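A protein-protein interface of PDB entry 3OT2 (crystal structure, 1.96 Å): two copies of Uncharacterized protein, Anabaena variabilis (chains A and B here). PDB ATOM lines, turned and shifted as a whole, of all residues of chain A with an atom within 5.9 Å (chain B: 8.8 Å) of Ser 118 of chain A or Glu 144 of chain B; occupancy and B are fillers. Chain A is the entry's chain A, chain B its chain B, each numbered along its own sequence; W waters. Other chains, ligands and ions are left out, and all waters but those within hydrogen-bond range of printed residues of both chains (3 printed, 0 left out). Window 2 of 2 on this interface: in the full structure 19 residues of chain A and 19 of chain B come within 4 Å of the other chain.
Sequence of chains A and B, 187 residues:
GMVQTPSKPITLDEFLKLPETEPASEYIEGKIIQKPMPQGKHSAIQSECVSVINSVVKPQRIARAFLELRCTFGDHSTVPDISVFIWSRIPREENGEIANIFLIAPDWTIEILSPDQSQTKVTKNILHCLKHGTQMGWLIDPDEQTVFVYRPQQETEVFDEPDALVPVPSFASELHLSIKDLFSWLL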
ATOM      1  N   PRO A  36      17.912  26.388 -10.529  1.00  0.00           N
ATOM      2  CA  PRO A  36      16.719  26.238  -9.677  1.00  0.00           C
ATOM      3  C   PRO A  36      17.032  26.465  -8.198  1.00  0.00           C
ATOM      4  O   PRO A  36      18.188  26.396  -7.766  1.00  0.00           O
ATOM      5  CB  PRO A  36      16.255  24.791  -9.943  1.00  0.00           C
ATOM      6  CG  PRO A  36      17.366  24.113 -10.519  1.00  0.00           C
ATOM      7  CD  PRO A  36      18.319  25.087 -11.110  1.00  0.00           C
ATOM      8  N   LEU A 113      18.813  16.476 -11.097  1.00  0.00           N
ATOM      9  CA  LEU A 113      17.519  17.111 -11.349  1.00  0.00           C
ATOM     10  C   LEU A 113      16.785  17.433 -10.066  1.00  0.00           C
ATOM     11  O   LEU A 113      16.935  16.753  -9.049  1.00  0.00           O
ATOM     12  CB  LEU A 113      16.620  16.225 -12.227  1.00  0.00           C
ATOM     13  CG  LEU A 113      17.127  15.905 -13.639  1.00  0.00           C
ATOM     14  CD1 LEU A 113      16.129  15.019 -14.339  1.00  0.00           C
ATOM     15  CD2 LEU A 113      17.390  17.197 -14.442  1.00  0.00           C
ATOM     16  N   SER A 114      16.000  18.501 -10.129  1.00  0.00           N
ATOM     17  CA  SER A 114      15.117  18.960  -9.055  1.00  0.00           C
ATOM     18  C   SER A 114      13.835  19.427  -9.758  1.00  0.00           C
ATOM     19  O   SER A 114      13.884  19.626 -10.976  1.00  0.00           O
ATOM     20  CB  SER A 114      15.784  20.020  -8.178  1.00  0.00           C
ATOM     21  OG  SER A 114      16.269  21.132  -8.899  1.00  0.00           O
ATOM     22  N   ASP A 116      12.147  22.130 -10.415  1.00  0.00           N
ATOM     23  CA  ASP A 116      12.120  23.327 -11.257  1.00  0.00           C
ATOM     24  C   ASP A 116      13.250  23.381 -12.304  1.00  0.00           C
ATOM     25  O   ASP A 116      13.315  24.329 -13.081  1.00  0.00           O
ATOM     26  CB  ASP A 116      12.161  24.570 -10.355  1.00  0.00           C
ATOM     27  CG  ASP A 116      10.931  24.700  -9.464  1.00  0.00           C
ATOM     28  OD1 ASP A 116       9.811  24.365  -9.933  1.00  0.00           O
ATOM     29  OD2 ASP A 116      11.089  25.127  -8.293  1.00  0.00           O
ATOM     30  N   GLN A 117      14.112  22.356 -12.347  1.00  0.00           N
ATOM     31  CA  GLN A 117      15.230  22.293 -13.271  1.00  0.00           C
ATOM     32  C   GLN A 117      14.758  21.944 -14.684  1.00  0.00           C
ATOM     33  O   GLN A 117      13.813  21.174 -14.855  1.00  0.00           O
ATOM     34  CB  GLN A 117      16.273  21.255 -12.763  1.00  0.00           C
ATOM     35  CG  GLN A 117      17.615  21.183 -13.528  1.00  0.00           C
ATOM     36  CD  GLN A 117      18.359  22.507 -13.650  1.00  0.00           C
ATOM     37  OE1 GLN A 117      17.864  23.466 -14.231  1.00  0.00           O
ATOM     38  NE2 GLN A 117      19.622  22.556 -13.242  1.00  0.00           N
ATOM     39  N   SER A 118      15.405  22.525 -15.701  1.00  0.00           N
ATOM     40  CA  SER A 118      15.127  22.176 -17.095  1.00  0.00           C
ATOM     41  C   SER A 118      16.061  21.029 -17.465  1.00  0.00           C
ATOM     42  O   SER A 118      17.271  21.233 -17.537  1.00  0.00           O
ATOM     43  CB  SER A 118      15.326  23.373 -18.024  1.00  0.00           C
ATOM     44  OG  SER A 118      15.388  22.937 -19.376  1.00  0.00           O
ATOM     45  N   GLN A 119      15.513  19.812 -17.657  1.00  0.00           N
ATOM     46  CA  GLN A 119      16.290  18.639 -18.060  1.00  0.00           C
ATOM     47  C   GLN A 119      16.933  18.870 -19.452  1.00  0.00           C
ATOM     48  O   GLN A 119      18.043  18.408 -19.693  1.00  0.00           O
ATOM     49  CB  GLN A 119      15.404  17.393 -18.062  1.00  0.00           C
ATOM     50  CG  GLN A 119      16.185  16.101 -18.330  1.00  0.00           C
ATOM     51  CD  GLN A 119      15.430  14.857 -17.945  1.00  0.00           C
ATOM     52  OE1 GLN A 119      14.396  14.916 -17.287  1.00  0.00           O
ATOM     53  NE2 GLN A 119      15.961  13.706 -18.305  1.00  0.00           N
ATOM     54  N   THR A 120      16.250  19.612 -20.354  1.00  0.00           N
ATOM     55  CA  THR A 120      16.805  19.924 -21.677  1.00  0.00           C
ATOM     56  C   THR A 120      18.058  20.794 -21.494  1.00  0.00           C
ATOM     57  O   THR A 120      19.086  20.456 -22.050  1.00  0.00           O
ATOM     58  CB  THR A 120      15.739  20.562 -22.549  1.00  0.00           C
ATOM     59  OG1 THR A 120      14.833  19.525 -22.924  1.00  0.00           O
ATOM     60  CG2 THR A 120      16.298  21.233 -23.813  1.00  0.00           C
ATOM     61  N   LYS A 121      17.980  21.870 -20.689  1.00  0.00           N
ATOM     62  CA  LYS A 121      19.114  22.762 -20.428  1.00  0.00           C
ATOM     63  C   LYS A 121      20.306  21.979 -19.849  1.00  0.00           C
ATOM     64  O   LYS A 121      21.435  22.160 -20.312  1.00  0.00           O
ATOM     65  CB  LYS A 121      18.703  23.893 -19.467  1.00  0.00           C
ATOM     66  CG  LYS A 121      19.834  24.820 -19.038  1.00  0.00           C
ATOM     67  CD  LYS A 121      19.412  25.763 -17.911  1.00  0.00           C
ATOM     68  CE  LYS A 121      19.404  25.043 -16.579  1.00  0.00           C
ATOM     69  NZ  LYS A 121      18.794  25.854 -15.482  1.00  0.00           N
ATOM     70  N   VAL A 122      20.045  21.106 -18.866  1.00  0.00           N
ATOM     71  CA  VAL A 122      21.065  20.283 -18.202  1.00  0.00           C
ATOM     72  C   VAL A 122      21.756  19.370 -19.200  1.00  0.00           C
ATOM     73  O   VAL A 122      22.984  19.252 -19.153  1.00  0.00           O
ATOM     74  CB  VAL A 122      20.431  19.477 -17.032  1.00  0.00           C
ATOM     75  CG1 VAL A 122      21.331  18.334 -16.612  1.00  0.00           C
ATOM     76  CG2 VAL A 122      20.176  20.384 -15.847  1.00  0.00           C
ATOM     77  N   THR A 123      20.977  18.714 -20.091  1.00  0.00           N
ATOM     78  CA  THR A 123      21.529  17.809 -21.116  1.00  0.00           C
ATOM     79  C   THR A 123      22.429  18.612 -22.056  1.00  0.00           C
ATOM     80  O   THR A 123      23.544  18.174 -22.318  1.00  0.00           O
ATOM     81  CB  THR A 123      20.411  17.060 -21.848  1.00  0.00           C
ATOM     82  OG1 THR A 123      19.734  16.300 -20.864  1.00  0.00           O
ATOM     83  CG2 THR A 123      20.950  16.109 -22.879  1.00  0.00           C
ATOM     84  N   LYS A 124      21.977  19.801 -22.498  1.00  0.00           N
ATOM     85  CA  LYS A 124      22.799  20.678 -23.346  1.00  0.00           C
ATOM     86  C   LYS A 124      24.110  21.043 -22.625  1.00  0.00           C
ATOM     87  O   LYS A 124      25.164  21.041 -23.253  1.00  0.00           O
ATOM     88  CB  LYS A 124      22.060  21.969 -23.705  1.00  0.00           C
ATOM     89  CG  LYS A 124      20.887  21.816 -24.653  1.00  0.00           C
ATOM     90  CD  LYS A 124      20.295  23.186 -24.859  1.00  0.00           C
ATOM     91  CE  LYS A 124      19.051  23.127 -25.670  1.00  0.00           C
ATOM     92  NZ  LYS A 124      18.562  24.496 -25.981  1.00  0.00           N
ATOM     93  N   LYS B  41      -0.432  22.220 -27.805  1.00  0.00           N
ATOM     94  CA  LYS B  41       0.887  22.405 -28.408  1.00  0.00           C
ATOM     95  C   LYS B  41       1.423  21.077 -28.943  1.00  0.00           C
ATOM     96  O   LYS B  41       1.841  20.999 -30.104  1.00  0.00           O
ATOM     97  CB  LYS B  41       1.859  23.038 -27.406  1.00  0.00           C
ATOM     98  CG  LYS B  41       1.701  24.560 -27.283  1.00  0.00           C
ATOM     99  CD  LYS B  41       2.345  25.180 -26.015  1.00  0.00           C
ATOM    100  CE  LYS B  41       3.857  25.257 -25.996  1.00  0.00           C
ATOM    101  NZ  LYS B  41       4.357  26.163 -24.926  1.00  0.00           N
ATOM    102  N   LEU B 113       7.717  16.258 -26.218  1.00  0.00           N
ATOM    103  CA  LEU B 113       7.428  16.538 -24.820  1.00  0.00           C
ATOM    104  C   LEU B 113       6.157  17.354 -24.664  1.00  0.00           C
ATOM    105  O   LEU B 113       5.806  18.152 -25.529  1.00  0.00           O
ATOM    106  CB  LEU B 113       8.581  17.276 -24.131  1.00  0.00           C
ATOM    107  CG  LEU B 113       9.932  16.540 -24.046  1.00  0.00           C
ATOM    108  CD1 LEU B 113      10.959  17.399 -23.368  1.00  0.00           C
ATOM    109  CD2 LEU B 113       9.807  15.177 -23.336  1.00  0.00           C
ATOM    110  N   GLN B 119      10.626  13.195 -19.298  1.00  0.00           N
ATOM    111  CA  GLN B 119      11.715  13.289 -20.274  1.00  0.00           C
ATOM    112  C   GLN B 119      12.713  12.119 -20.085  1.00  0.00           C
ATOM    113  O   GLN B 119      13.252  11.620 -21.076  1.00  0.00           O
ATOM    114  CB  GLN B 119      12.424  14.644 -20.163  1.00  0.00           C
ATOM    115  CG  GLN B 119      13.445  14.888 -21.268  1.00  0.00           C
ATOM    116  CD  GLN B 119      13.843  16.329 -21.385  1.00  0.00           C
ATOM    117  OE1 GLN B 119      13.215  17.241 -20.848  1.00  0.00           O
ATOM    118  NE2 GLN B 119      14.889  16.582 -22.110  1.00  0.00           N
ATOM    119  N   LEU B 139      13.864  13.760 -30.173  1.00  0.00           N
ATOM    120  CA  LEU B 139      13.226  14.184 -28.928  1.00  0.00           C
ATOM    121  C   LEU B 139      12.980  15.669 -29.090  1.00  0.00           C
ATOM    122  O   LEU B 139      13.922  16.454 -29.056  1.00  0.00           O
ATOM    123  CB  LEU B 139      14.052  13.846 -27.671  1.00  0.00           C
ATOM    124  CG  LEU B 139      13.278  13.799 -26.325  1.00  0.00           C
ATOM    125  CD1 LEU B 139      14.152  13.286 -25.216  1.00  0.00           C
ATOM    126  CD2 LEU B 139      12.766  15.162 -25.903  1.00  0.00           C
ATOM    127  N   ILE B 140      11.723  16.041 -29.365  1.00  0.00           N
ATOM    128  CA  ILE B 140      11.320  17.429 -29.587  1.00  0.00           C
ATOM    129  C   ILE B 140      10.855  18.032 -28.266  1.00  0.00           C
ATOM    130  O   ILE B 140       9.998  17.466 -27.591  1.00  0.00           O
ATOM    131  CB  ILE B 140      10.205  17.536 -30.683  1.00  0.00           C
ATOM    132  CG1 ILE B 140      10.691  16.971 -32.050  1.00  0.00           C
ATOM    133  CG2 ILE B 140       9.695  18.982 -30.806  1.00  0.00           C
ATOM    134  CD1 ILE B 140       9.587  16.755 -33.111  1.00  0.00           C
ATOM    135  N   ASP B 141      11.421  19.179 -27.909  1.00  0.00           N
ATOM    136  CA  ASP B 141      11.053  19.922 -26.704  1.00  0.00           C
ATOM    137  C   ASP B 141      10.418  21.253 -27.151  1.00  0.00           C
ATOM    138  O   ASP B 141      11.158  22.217 -27.396  1.00  0.00           O
ATOM    139  CB  ASP B 141      12.273  20.167 -25.803  1.00  0.00           C
ATOM    140  CG  ASP B 141      11.928  20.894 -24.506  1.00  0.00           C
ATOM    141  OD1 ASP B 141      10.856  21.542 -24.447  1.00  0.00           O
ATOM    142  OD2 ASP B 141      12.697  20.782 -23.544  1.00  0.00           O
ATOM    143  N   PRO B 142       9.064  21.328 -27.257  1.00  0.00           N
ATOM    144  CA  PRO B 142       8.427  22.571 -27.747  1.00  0.00           C
ATOM    145  C   PRO B 142       8.790  23.799 -26.914  1.00  0.00           C
ATOM    146  O   PRO B 142       9.167  24.814 -27.488  1.00  0.00           O
ATOM    147  CB  PRO B 142       6.936  22.250 -27.670  1.00  0.00           C
ATOM    148  CG  PRO B 142       6.870  20.771 -27.842  1.00  0.00           C
ATOM    149  CD  PRO B 142       8.053  20.270 -27.047  1.00  0.00           C
ATOM    150  N   ASP B 143       8.766  23.684 -25.581  1.00  0.00           N
ATOM    151  CA  ASP B 143       9.070  24.789 -24.671  1.00  0.00           C
ATOM    152  C   ASP B 143      10.458  25.356 -24.886  1.00  0.00           C
ATOM    153  O   ASP B 143      10.613  26.569 -24.831  1.00  0.00           O
ATOM    154  CB  ASP B 143       8.898  24.364 -23.193  1.00  0.00           C
ATOM    155  CG  ASP B 143       7.457  24.113 -22.740  1.00  0.00           C
ATOM    156  OD1 ASP B 143       6.522  24.556 -23.441  1.00  0.00           O
ATOM    157  OD2 ASP B 143       7.270  23.468 -21.691  1.00  0.00           O
ATOM    158  N   GLU B 144      11.471  24.506 -25.118  1.00  0.00           N
ATOM    159  CA  GLU B 144      12.832  24.971 -25.317  1.00  0.00           C
ATOM    160  C   GLU B 144      13.163  25.131 -26.804  1.00  0.00           C
ATOM    161  O   GLU B 144      14.296  25.481 -27.127  1.00  0.00           O
ATOM    162  CB  GLU B 144      13.827  24.000 -24.667  1.00  0.00           C
ATOM    163  CG  GLU B 144      13.672  23.884 -23.162  1.00  0.00           C
ATOM    164  CD  GLU B 144      14.565  24.760 -22.311  1.00  0.00           C
ATOM    165  OE1 GLU B 144      15.346  25.561 -22.871  1.00  0.00           O
ATOM    166  OE2 GLU B 144      14.475  24.652 -21.069  1.00  0.00           O
ATOM    167  N   GLN B 145      12.205  24.852 -27.700  1.00  0.00           N
ATOM    168  CA  GLN B 145      12.393  24.918 -29.167  1.00  0.00           C
ATOM    169  C   GLN B 145      13.708  24.214 -29.544  1.00  0.00           C
ATOM    170  O   GLN B 145      14.575  24.760 -30.249  1.00  0.00           O
ATOM    171  CB  GLN B 145      12.331  26.360 -29.693  1.00  0.00           C
ATOM    172  CG  GLN B 145      10.945  26.987 -29.478  1.00  0.00           C
ATOM    173  CD  GLN B 145      10.858  28.422 -29.926  1.00  0.00           C
ATOM    174  OE1 GLN B 145      11.312  28.796 -31.008  1.00  0.00           O
ATOM    175  NE2 GLN B 145      10.251  29.261 -29.104  1.00  0.00           N
ATOM    176  N   THR B 146      13.843  22.984 -29.025  1.00  0.00           N
ATOM    177  CA  THR B 146      15.035  22.171 -29.172  1.00  0.00           C
ATOM    178  C   THR B 146      14.670  20.799 -29.664  1.00  0.00           C
ATOM    179  O   THR B 146      13.601  20.274 -29.333  1.00  0.00           O
ATOM    180  CB  THR B 146      15.749  22.103 -27.801  1.00  0.00           C
ATOM    181  OG1 THR B 146      16.209  23.410 -27.445  1.00  0.00           O
ATOM    182  CG2 THR B 146      16.945  21.126 -27.793  1.00  0.00           C
ATOM    183  N   VAL B 147      15.562  20.218 -30.475  1.00  0.00           N
ATOM    184  CA  VAL B 147      15.427  18.834 -30.902  1.00  0.00           C
ATOM    185  C   VAL B 147      16.716  18.096 -30.535  1.00  0.00           C
ATOM    186  O   VAL B 147      17.803  18.523 -30.936  1.00  0.00           O
ATOM    187  CB  VAL B 147      15.048  18.606 -32.396  1.00  0.00           C
ATOM    188  CG1 VAL B 147      14.851  17.117 -32.691  1.00  0.00           C
ATOM    189  CG2 VAL B 147      13.798  19.383 -32.764  1.00  0.00           C
ATOM    190  N   PHE B 148      16.589  16.989 -29.776  1.00  0.00           N
ATOM    191  CA  PHE B 148      17.720  16.091 -29.522  1.00  0.00           C
ATOM    192  C   PHE B 148      17.649  14.980 -30.554  1.00  0.00           C
ATOM    193  O   PHE B 148      16.566  14.418 -30.788  1.00  0.00           O
ATOM    194  CB  PHE B 148      17.707  15.508 -28.110  1.00  0.00           C
ATOM    195  CG  PHE B 148      17.942  16.494 -26.995  1.00  0.00           C
ATOM    196  CD1 PHE B 148      19.199  17.037 -26.780  1.00  0.00           C
ATOM    197  CD2 PHE B 148      16.907  16.883 -26.162  1.00  0.00           C
ATOM    198  CE1 PHE B 148      19.433  17.921 -25.714  1.00  0.00           C
ATOM    199  CE2 PHE B 148      17.137  17.778 -25.099  1.00  0.00           C
ATOM    200  CZ  PHE B 148      18.402  18.287 -24.883  1.00  0.00           C
ATOM    201  N   VAL B 158      22.396  18.077 -30.426  1.00  0.00           N
ATOM    202  CA  VAL B 158      21.451  19.152 -30.070  1.00  0.00           C
ATOM    203  C   VAL B 158      21.247  20.095 -31.230  1.00  0.00           C
ATOM    204  O   VAL B 158      22.227  20.580 -31.796  1.00  0.00           O
ATOM    205  CB  VAL B 158      21.937  19.983 -28.831  1.00  0.00           C
ATOM    206  CG1 VAL B 158      20.796  20.859 -28.297  1.00  0.00           C
ATOM    207  CG2 VAL B 158      22.481  19.092 -27.735  1.00  0.00           C
ATOM    208  N   PHE B 159      19.975  20.426 -31.525  1.00  0.00           N
ATOM    209  CA  PHE B 159      19.610  21.377 -32.583  1.00  0.00           C
ATOM    210  C   PHE B 159      18.675  22.415 -31.964  1.00  0.00           C
ATOM    211  O   PHE B 159      17.624  22.050 -31.415  1.00  0.00           O
ATOM    212  CB  PHE B 159      18.965  20.646 -33.806  1.00  0.00           C
ATOM    213  CG  PHE B 159      20.014  19.763 -34.448  1.00  0.00           C
ATOM    214  CD1 PHE B 159      20.900  20.282 -35.386  1.00  0.00           C
ATOM    215  CD2 PHE B 159      20.197  18.446 -34.022  1.00  0.00           C
ATOM    216  CE1 PHE B 159      21.942  19.494 -35.902  1.00  0.00           C
ATOM    217  CE2 PHE B 159      21.247  17.673 -34.523  1.00  0.00           C
ATOM    218  CZ  PHE B 159      22.133  18.210 -35.435  1.00  0.00           C
ATOM    219  N   ASP B 160      19.093  23.699 -31.974  1.00  0.00           N
ATOM    220  CA  ASP B 160      18.234  24.758 -31.434  1.00  0.00           C
ATOM    221  C   ASP B 160      18.419  26.114 -32.141  1.00  0.00           C
ATOM    222  O   ASP B 160      17.759  27.074 -31.748  1.00  0.00           O
ATOM    223  CB  ASP B 160      18.409  24.919 -29.921  1.00  0.00           C
ATOM    224  CG  ASP B 160      19.792  25.259 -29.435  1.00  0.00           C
ATOM    225  OD1 ASP B 160      20.548  25.903 -30.185  1.00  0.00           O
ATOM    226  OD2 ASP B 160      20.110  24.901 -28.306  1.00  0.00           O
ATOM    227  N   GLU B 161      19.306  26.204 -33.152  1.00  0.00           N
ATOM    228  CA  GLU B 161      19.495  27.434 -33.930  1.00  0.00           C
ATOM    229  C   GLU B 161      18.341  27.536 -34.911  1.00  0.00           C
ATOM    230  O   GLU B 161      18.051  26.540 -35.579  1.00  0.00           O
ATOM    231  CB  GLU B 161      20.856  27.469 -34.654  1.00  0.00           C
ATOM    232  CG  GLU B 161      22.031  27.728 -33.724  1.00  0.00           C
ATOM    233  CD  GLU B 161      22.089  29.114 -33.109  1.00  0.00           C
ATOM    234  OE1 GLU B 161      22.347  30.088 -33.855  1.00  0.00           O
ATOM    235  OE2 GLU B 161      21.885  29.223 -31.878  1.00  0.00           O
ATOM    236  N   ILE B 179      14.664  24.269 -37.570  1.00  0.00           N
ATOM    237  CA  ILE B 179      14.160  24.449 -36.211  1.00  0.00           C
ATOM    238  C   ILE B 179      13.004  25.471 -36.261  1.00  0.00           C
ATOM    239  O   ILE B 179      11.921  25.192 -35.734  1.00  0.00           O
ATOM    240  CB  ILE B 179      15.319  24.871 -35.263  1.00  0.00           C
ATOM    241  CG1 ILE B 179      16.251  23.670 -34.948  1.00  0.00           C
ATOM    242  CG2 ILE B 179      14.825  25.569 -33.955  1.00  0.00           C
ATOM    243  CD1 ILE B 179      15.603  22.528 -34.010  1.00  0.00           C
ATOM    244  N   PHE B 183       8.993  24.657 -35.045  1.00  0.00           N
ATOM    245  CA  PHE B 183       8.314  25.306 -33.932  1.00  0.00           C
ATOM    246  C   PHE B 183       7.340  26.383 -34.376  1.00  0.00           C
ATOM    247  O   PHE B 183       6.507  26.780 -33.556  1.00  0.00           O
ATOM    248  CB  PHE B 183       9.320  25.797 -32.886  1.00  0.00           C
ATOM    249  CG  PHE B 183      10.050  24.592 -32.331  1.00  0.00           C
ATOM    250  CD1 PHE B 183       9.389  23.669 -31.517  1.00  0.00           C
ATOM    251  CD2 PHE B 183      11.364  24.325 -32.702  1.00  0.00           C
ATOM    252  CE1 PHE B 183      10.033  22.520 -31.071  1.00  0.00           C
ATOM    253  CE2 PHE B 183      12.009  23.170 -32.255  1.00  0.00           C
ATOM    254  CZ  PHE B 183      11.338  22.273 -31.442  1.00  0.00           C
ATOM    255  N   LEU B 186       3.481  25.841 -33.886  1.00  0.00           N
ATOM    256  CA  LEU B 186       2.850  26.250 -32.634  1.00  0.00           C
ATOM    257  C   LEU B 186       2.098  27.569 -32.786  1.00  0.00           C
ATOM    258  O   LEU B 186       1.257  27.899 -31.941  1.00  0.00           O
ATOM    259  CB  LEU B 186       3.908  26.418 -31.540  1.00  0.00           C
ATOM    260  CG  LEU B 186       4.658  25.185 -31.073  1.00  0.00           C
ATOM    261  CD1 LEU B 186       5.683  25.569 -30.050  1.00  0.00           C
ATOM    262  CD2 LEU B 186       3.712  24.152 -30.518  1.00  0.00           C
HETATM  263  O   HOH W   1      13.357  19.850 -20.005  1.00  0.00           O
HETATM  264  O   HOH W   2      12.257  13.345 -16.593  1.00  0.00           O
HETATM  265  O   HOH W   3      17.044  27.269 -26.411  1.00  0.00           O
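Along chain A the printed residues that touch a printed residue of chain B span positions 118 to 124.
Among the printed residues, Asp or Glu carboxylates within 4 Å of a Lys or Arg side-chain nitrogen of the other chain: Lys 124 of chain A with Asp 160 of chain B.
The side-chain hydroxyl of Ser 118 of chain A lies within hydrogen-bond range of the side-chain carboxylate of Glu 144 of chain B (2.6 Å).
The side-chain amide nitrogen of Gln 119 of chain B sits at hydrogen-bond distance from the side-chain hydroxyl of Thr 120 of chain A (3.1 Å).
The side-chain carboxylate of Asp 141 of chain B sits at hydrogen-bond distance from the side-chain hydroxyl of Thr 120 of chain A (2.6 Å).
NZ of Lys 124 of chain A sits at hydrogen-bond distance from OG1 of Thr 146 of chain B, 3.0 Å away.
NZ of Lys 124 of chain A is in salt-bridge range of OD2 of Asp 160 of chain B, 2.8 Å away.
Ser 118 of chain A touches just one residue of chain B: Glu 144 (2.6 Å).
Of the printed residues of chain B, Thr 120 of chain A touches Gln 119, Asp 141, Glu 144 and Phe 148.
Lys 41 of chain B touches none of the printed residues of chain A.
Of the printed residues of chain A, Gln 119 of chain B touches Gln 119 and Thr 120.
Printed residues of chain A within 4 Å of Asp 141 of chain B: Thr 120.
Glu 144 of chain B touches just these residues of chain A: Ser 118 (2.6 Å) and Thr 120 (3.8 Å).
Val 147 of chain B touches none of the printed residues of chain A.
Of the printed residues of chain A, Phe 148 of chain B touches Thr 120 and Thr 123.
Of the printed residues of chain A, Val 158 of chain B touches Lys 124 (3.8 Å).
The nearest residue of chain B that does not touch Ser 118 of chain A is Asp 141 of chain B (5.4 Å).
The nearest printed residue of chain A that does not touch Asp 141 of chain B is Ser 118 of chain A (5.4 Å).
Among the printed residues, pairs that only touch across the chains: Gln 119 of chain A with Gln 119 of chain B (3.5 Å), Thr 120 of chain A with Glu 144 of chain B (3.8 Å), Thr 120 of chain A with Phe 148 of chain B (3.6 Å), Thr 123 of chain A with Phe 148 of chain B (3.7 Å) and Lys 124 of chain A with Val 158 of chain B (3.8 Å).
The side-chain hydroxyl (OG) of Ser 118 of chain A is in hydrogen-bond range of the backbone NH (N) of Lys 121 of chain A.
O of Gln 119 of chain A is in hydrogen-bond range of OG1 of Thr 123 of chain A, 2.9 Å away.
N of Phe 148 of chain B lies within hydrogen-bond range of O of Leu 139 of chain B, at 2.8 Å.
The side-chain carboxylate (OD1) of Asp 141 of chain B lies within hydrogen-bond range of the backbone NH (N) of Asp 143 of chain B, 3.2 Å away.
The side-chain carboxylate (OD1) of Asp 141 of chain B is in hydrogen-bond range of the backbone NH (N) of Glu 144 of chain B (3.1 Å).
The backbone NH of Asp 141 of chain B is in hydrogen-bond range of the backbone carbonyl oxygen of Thr 146 of chain B (2.8 Å).
Water W2 bridges OE1 of Gln 119 of chain A (2.7 Å) and N of Gln 119 of chain B (3.2 Å).
Water W1 lies within hydrogen-bond range of the side-chain amide oxygen (OE1) of Gln 119 of chain B (2.7 Å), the backbone NH (N) of Thr 120 of chain A (2.9 Å) and the backbone NH (N) of Gln 119 of chain A (3.2 Å).
Water W3 bridges the side-chain amino group (NZ) of Lys 124 of chain A (3.2 Å) and the backbone carbonyl oxygen (O) of Glu 144 of chain B (3.4 Å).
Gln 119 of chain A touches its own counterpart, Gln 119 of chain B.
Positions printed for both chains: 113 and 119.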
